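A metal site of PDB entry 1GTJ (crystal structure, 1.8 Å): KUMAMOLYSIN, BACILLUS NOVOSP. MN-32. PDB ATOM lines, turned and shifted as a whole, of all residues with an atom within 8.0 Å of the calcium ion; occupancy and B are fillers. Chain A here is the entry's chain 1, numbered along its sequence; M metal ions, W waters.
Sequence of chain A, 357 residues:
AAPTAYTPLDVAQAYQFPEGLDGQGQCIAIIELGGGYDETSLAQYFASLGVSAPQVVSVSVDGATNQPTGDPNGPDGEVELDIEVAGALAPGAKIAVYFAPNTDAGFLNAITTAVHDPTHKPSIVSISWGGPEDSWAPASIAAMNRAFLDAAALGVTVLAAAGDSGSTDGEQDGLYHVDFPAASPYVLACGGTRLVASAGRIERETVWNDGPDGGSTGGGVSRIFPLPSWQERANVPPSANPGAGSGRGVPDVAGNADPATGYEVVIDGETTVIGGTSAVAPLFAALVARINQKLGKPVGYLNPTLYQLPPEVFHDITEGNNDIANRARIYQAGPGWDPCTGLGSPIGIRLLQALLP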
ATOM      1  N   VAL A 207      32.744 -28.540  16.531  1.00  0.00           N
ATOM      2  CA  VAL A 207      32.911 -27.448  17.499  1.00  0.00           C
ATOM      3  C   VAL A 207      34.192 -27.667  18.304  1.00  0.00           C
ATOM      4  O   VAL A 207      34.496 -28.790  18.729  1.00  0.00           O
ATOM      5  CB  VAL A 207      31.733 -27.378  18.534  1.00  0.00           C
ATOM      6  CG1 VAL A 207      31.934 -26.173  19.475  1.00  0.00           C
ATOM      7  CG2 VAL A 207      30.402 -27.242  17.803  1.00  0.00           C
ATOM      8  N   HIS A 315      30.501 -23.667   5.061  1.00  0.00           N
ATOM      9  CA  HIS A 315      30.588 -25.087   5.377  1.00  0.00           C
ATOM     10  C   HIS A 315      29.912 -25.147   6.754  1.00  0.00           C
ATOM     11  O   HIS A 315      30.392 -24.549   7.723  1.00  0.00           O
ATOM     12  CB  HIS A 315      32.050 -25.536   5.457  1.00  0.00           C
ATOM     13  CG  HIS A 315      32.199 -26.964   5.872  1.00  0.00           C
ATOM     14  ND1 HIS A 315      32.672 -27.335   7.116  1.00  0.00           N
ATOM     15  CD2 HIS A 315      31.860 -28.121   5.246  1.00  0.00           C
ATOM     16  CE1 HIS A 315      32.617 -28.648   7.235  1.00  0.00           C
ATOM     17  NE2 HIS A 315      32.125 -29.152   6.120  1.00  0.00           N
ATOM     18  N   ASP A 316      28.794 -25.863   6.818  1.00  0.00           N
ATOM     19  CA  ASP A 316      27.990 -25.989   8.027  1.00  0.00           C
ATOM     20  C   ASP A 316      28.612 -26.931   9.056  1.00  0.00           C
ATOM     21  O   ASP A 316      28.912 -28.078   8.725  1.00  0.00           O
ATOM     22  CB  ASP A 316      26.590 -26.526   7.621  1.00  0.00           C
ATOM     23  CG  ASP A 316      25.556 -26.370   8.718  1.00  0.00           C
ATOM     24  OD1 ASP A 316      25.935 -25.982   9.808  1.00  0.00           O
ATOM     25  OD2 ASP A 316      24.370 -26.650   8.465  1.00  0.00           O
ATOM     26  N   ILE A 317      28.858 -26.440  10.283  1.00  0.00           N
ATOM     27  CA  ILE A 317      29.393 -27.333  11.323  1.00  0.00           C
ATOM     28  C   ILE A 317      28.136 -27.789  12.033  1.00  0.00           C
ATOM     29  O   ILE A 317      27.322 -26.976  12.424  1.00  0.00           O
ATOM     30  CB  ILE A 317      30.323 -26.613  12.333  1.00  0.00           C
ATOM     31  CG1 ILE A 317      31.695 -26.328  11.709  1.00  0.00           C
ATOM     32  CG2 ILE A 317      30.583 -27.547  13.535  1.00  0.00           C
ATOM     33  CD1 ILE A 317      31.735 -25.335  10.598  1.00  0.00           C
ATOM     34  N   THR A 318      27.954 -29.095  12.200  1.00  0.00           N
ATOM     35  CA  THR A 318      26.719 -29.602  12.806  1.00  0.00           C
ATOM     36  C   THR A 318      26.930 -30.465  14.033  1.00  0.00           C
ATOM     37  O   THR A 318      25.955 -30.852  14.707  1.00  0.00           O
ATOM     38  CB  THR A 318      25.964 -30.469  11.803  1.00  0.00           C
ATOM     39  OG1 THR A 318      26.787 -31.590  11.461  1.00  0.00           O
ATOM     40  CG2 THR A 318      25.660 -29.687  10.522  1.00  0.00           C
ATOM     41  N   GLU A 319      28.192 -30.755  14.325  1.00  0.00           N
ATOM     42  CA  GLU A 319      28.520 -31.621  15.440  1.00  0.00           C
ATOM     43  C   GLU A 319      29.345 -30.969  16.530  1.00  0.00           C
ATOM     44  O   GLU A 319      30.325 -30.262  16.231  1.00  0.00           O
ATOM     45  CB  GLU A 319      29.262 -32.847  14.910  1.00  0.00           C
ATOM     46  N   GLN A 332      24.492 -26.262  21.728  1.00  0.00           N
ATOM     47  CA  GLN A 332      24.892 -27.305  20.770  1.00  0.00           C
ATOM     48  C   GLN A 332      24.902 -26.878  19.287  1.00  0.00           C
ATOM     49  O   GLN A 332      24.087 -26.049  18.863  1.00  0.00           O
ATOM     50  CB  GLN A 332      23.936 -28.479  20.939  1.00  0.00           C
ATOM     51  CG  GLN A 332      24.458 -29.836  20.534  1.00  0.00           C
ATOM     52  CD  GLN A 332      23.524 -30.928  21.026  1.00  0.00           C
ATOM     53  OE1 GLN A 332      22.356 -30.992  20.616  1.00  0.00           O
ATOM     54  NE2 GLN A 332      24.016 -31.778  21.908  1.00  0.00           N
ATOM     55  N   ALA A 333      25.804 -27.466  18.498  1.00  0.00           N
ATOM     56  CA  ALA A 333      25.863 -27.180  17.056  1.00  0.00           C
ATOM     57  C   ALA A 333      24.753 -27.988  16.388  1.00  0.00           C
ATOM     58  O   ALA A 333      24.281 -28.996  16.937  1.00  0.00           O
ATOM     59  CB  ALA A 333      27.221 -27.585  16.469  1.00  0.00           C
ATOM     60  N   GLY A 334      24.353 -27.562  15.213  1.00  0.00           N
ATOM     61  CA  GLY A 334      23.316 -28.290  14.493  1.00  0.00           C
ATOM     62  C   GLY A 334      23.202 -27.761  13.082  1.00  0.00           C
ATOM     63  O   GLY A 334      24.024 -26.970  12.652  1.00  0.00           O
ATOM     64  N   PRO A 335      22.228 -28.223  12.302  1.00  0.00           N
ATOM     65  CA  PRO A 335      22.129 -27.697  10.934  1.00  0.00           C
ATOM     66  C   PRO A 335      21.772 -26.206  10.939  1.00  0.00           C
ATOM     67  O   PRO A 335      20.955 -25.760  11.748  1.00  0.00           O
ATOM     68  CB  PRO A 335      21.020 -28.556  10.310  1.00  0.00           C
ATOM     69  CG  PRO A 335      20.246 -29.071  11.473  1.00  0.00           C
ATOM     70  CD  PRO A 335      21.282 -29.329  12.525  1.00  0.00           C
ATOM     71  N   GLY A 336      22.380 -25.468  10.020  1.00  0.00           N
ATOM     72  CA  GLY A 336      22.114 -24.038   9.929  1.00  0.00           C
ATOM     73  C   GLY A 336      22.896 -23.264  10.993  1.00  0.00           C
ATOM     74  O   GLY A 336      23.818 -23.796  11.560  1.00  0.00           O
ATOM     75  N   TRP A 337      22.530 -22.015  11.241  1.00  0.00           N
ATOM     76  CA  TRP A 337      23.227 -21.228  12.240  1.00  0.00           C
ATOM     77  C   TRP A 337      23.093 -21.892  13.619  1.00  0.00           C
ATOM     78  O   TRP A 337      22.063 -22.499  13.919  1.00  0.00           O
ATOM     79  CB  TRP A 337      22.573 -19.830  12.303  1.00  0.00           C
ATOM     80  CG  TRP A 337      23.309 -18.870  13.181  1.00  0.00           C
ATOM     81  CD1 TRP A 337      24.273 -17.984  12.797  1.00  0.00           C
ATOM     82  CD2 TRP A 337      23.215 -18.781  14.606  1.00  0.00           C
ATOM     83  NE1 TRP A 337      24.803 -17.354  13.907  1.00  0.00           N
ATOM     84  CE2 TRP A 337      24.165 -17.832  15.026  1.00  0.00           C
ATOM     85  CE3 TRP A 337      22.413 -19.428  15.568  1.00  0.00           C
ATOM     86  CZ2 TRP A 337      24.348 -17.500  16.380  1.00  0.00           C
ATOM     87  CZ3 TRP A 337      22.588 -19.099  16.915  1.00  0.00           C
ATOM     88  CH2 TRP A 337      23.549 -18.137  17.306  1.00  0.00           C
ATOM     89  N   ASP A 338      24.144 -21.823  14.452  1.00  0.00           N
ATOM     90  CA  ASP A 338      24.014 -22.320  15.817  1.00  0.00           C
ATOM     91  C   ASP A 338      24.884 -21.445  16.721  1.00  0.00           C
ATOM     92  O   ASP A 338      25.760 -20.714  16.230  1.00  0.00           O
ATOM     93  CB  ASP A 338      24.385 -23.811  15.954  1.00  0.00           C
ATOM     94  CG  ASP A 338      25.749 -24.107  15.439  1.00  0.00           C
ATOM     95  OD1 ASP A 338      26.721 -23.614  16.013  1.00  0.00           O
ATOM     96  OD2 ASP A 338      25.844 -24.833  14.444  1.00  0.00           O
ATOM     97  N   PRO A 339      24.659 -21.514  18.038  1.00  0.00           N
ATOM     98  CA  PRO A 339      25.439 -20.685  18.958  1.00  0.00           C
ATOM     99  C   PRO A 339      26.839 -21.193  19.288  1.00  0.00           C
ATOM    100  O   PRO A 339      27.408 -20.857  20.340  1.00  0.00           O
ATOM    101  CB  PRO A 339      24.504 -20.535  20.190  1.00  0.00           C
ATOM    102  CG  PRO A 339      23.175 -21.293  19.744  1.00  0.00           C
ATOM    103  CD  PRO A 339      23.651 -22.294  18.757  1.00  0.00           C
ATOM    104  N   CYS A 340      27.411 -22.016  18.407  1.00  0.00           N
ATOM    105  CA  CYS A 340      28.772 -22.498  18.636  1.00  0.00           C
ATOM    106  C   CYS A 340      29.623 -22.044  17.477  1.00  0.00           C
ATOM    107  O   CYS A 340      30.768 -21.673  17.669  1.00  0.00           O
ATOM    108  CB  CYS A 340      28.882 -24.027  18.681  1.00  0.00           C
ATOM    109  SG  CYS A 340      27.938 -24.815  19.967  1.00  0.00           S
ATOM    110  N   THR A 341      29.037 -22.099  16.279  1.00  0.00           N
ATOM    111  CA  THR A 341      29.780 -21.783  15.068  1.00  0.00           C
ATOM    112  C   THR A 341      29.104 -20.833  14.102  1.00  0.00           C
ATOM    113  O   THR A 341      29.635 -20.572  13.027  1.00  0.00           O
ATOM    114  CB  THR A 341      30.129 -23.080  14.326  1.00  0.00           C
ATOM    115  OG1 THR A 341      28.924 -23.757  13.963  1.00  0.00           O
ATOM    116  CG2 THR A 341      30.976 -24.014  15.222  1.00  0.00           C
ATOM    117  N   GLY A 342      27.943 -20.298  14.474  1.00  0.00           N
ATOM    118  CA  GLY A 342      27.296 -19.369  13.559  1.00  0.00           C
ATOM    119  C   GLY A 342      26.984 -20.018  12.232  1.00  0.00           C
ATOM    120  O   GLY A 342      26.543 -21.168  12.200  1.00  0.00           O
ATOM    121  N   LEU A 343      27.225 -19.289  11.142  1.00  0.00           N
ATOM    122  CA  LEU A 343      26.976 -19.745   9.765  1.00  0.00           C
ATOM    123  C   LEU A 343      27.958 -20.835   9.344  1.00  0.00           C
ATOM    124  O   LEU A 343      27.779 -21.506   8.310  1.00  0.00           O
ATOM    125  CB  LEU A 343      27.057 -18.535   8.815  1.00  0.00           C
ATOM    126  CG  LEU A 343      26.069 -17.401   9.099  1.00  0.00           C
ATOM    127  CD1 LEU A 343      26.371 -16.221   8.145  1.00  0.00           C
ATOM    128  CD2 LEU A 343      24.617 -17.882   8.896  1.00  0.00           C
ATOM    129  N   GLY A 344      28.976 -21.036  10.168  1.00  0.00           N
ATOM    130  CA  GLY A 344      29.995 -22.046   9.886  1.00  0.00           C
ATOM    131  C   GLY A 344      31.283 -21.416   9.374  1.00  0.00           C
ATOM    132  O   GLY A 344      31.550 -20.244   9.624  1.00  0.00           O
ATOM    133  N   SER A 345      32.102 -22.199   8.699  1.00  0.00           N
ATOM    134  CA  SER A 345      33.342 -21.657   8.162  1.00  0.00           C
ATOM    135  C   SER A 345      33.111 -21.183   6.725  1.00  0.00           C
ATOM    136  O   SER A 345      32.452 -21.847   5.919  1.00  0.00           O
ATOM    137  CB  SER A 345      34.464 -22.715   8.237  1.00  0.00           C
ATOM    138  OG  SER A 345      34.100 -23.913   7.549  1.00  0.00           O
HETATM  139 CA    CA M   1      25.599 -25.321  12.078  1.00  0.00          CA
HETATM  140  O   HOH W   1      27.440 -23.593  11.821  1.00  0.00           O
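The calcium ion is bound by the backbone carbonyl oxygen (O) of Gly 334, the side-chain carboxylate (OD1) of Asp 316, the backbone carbonyl oxygen (O) of Gly 336, the backbone carbonyl oxygen (O) of Ile 317, the side-chain carboxylate (OD2) of Asp 338 and water W1.
The calcium ion has six donor atoms within binding distance.
Of the 20 residues printed, 5 come within 4 Å of the calcium ion.
The backbone NH (N) of Thr 341 sits at hydrogen-bond distance from the side-chain carboxylate (OD1) of Asp 338 (2.8 Å).
N of Cys 340 is in hydrogen-bond range of OD1 of Asp 338 (3.0 Å).
Water W1 lies within hydrogen-bond range of the side-chain hydroxyl of Thr 341 (2.6 Å), the backbone carbonyl oxygen of Gly 342 (2.6 Å) and the backbone NH of Gly 344 (3.4 Å).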
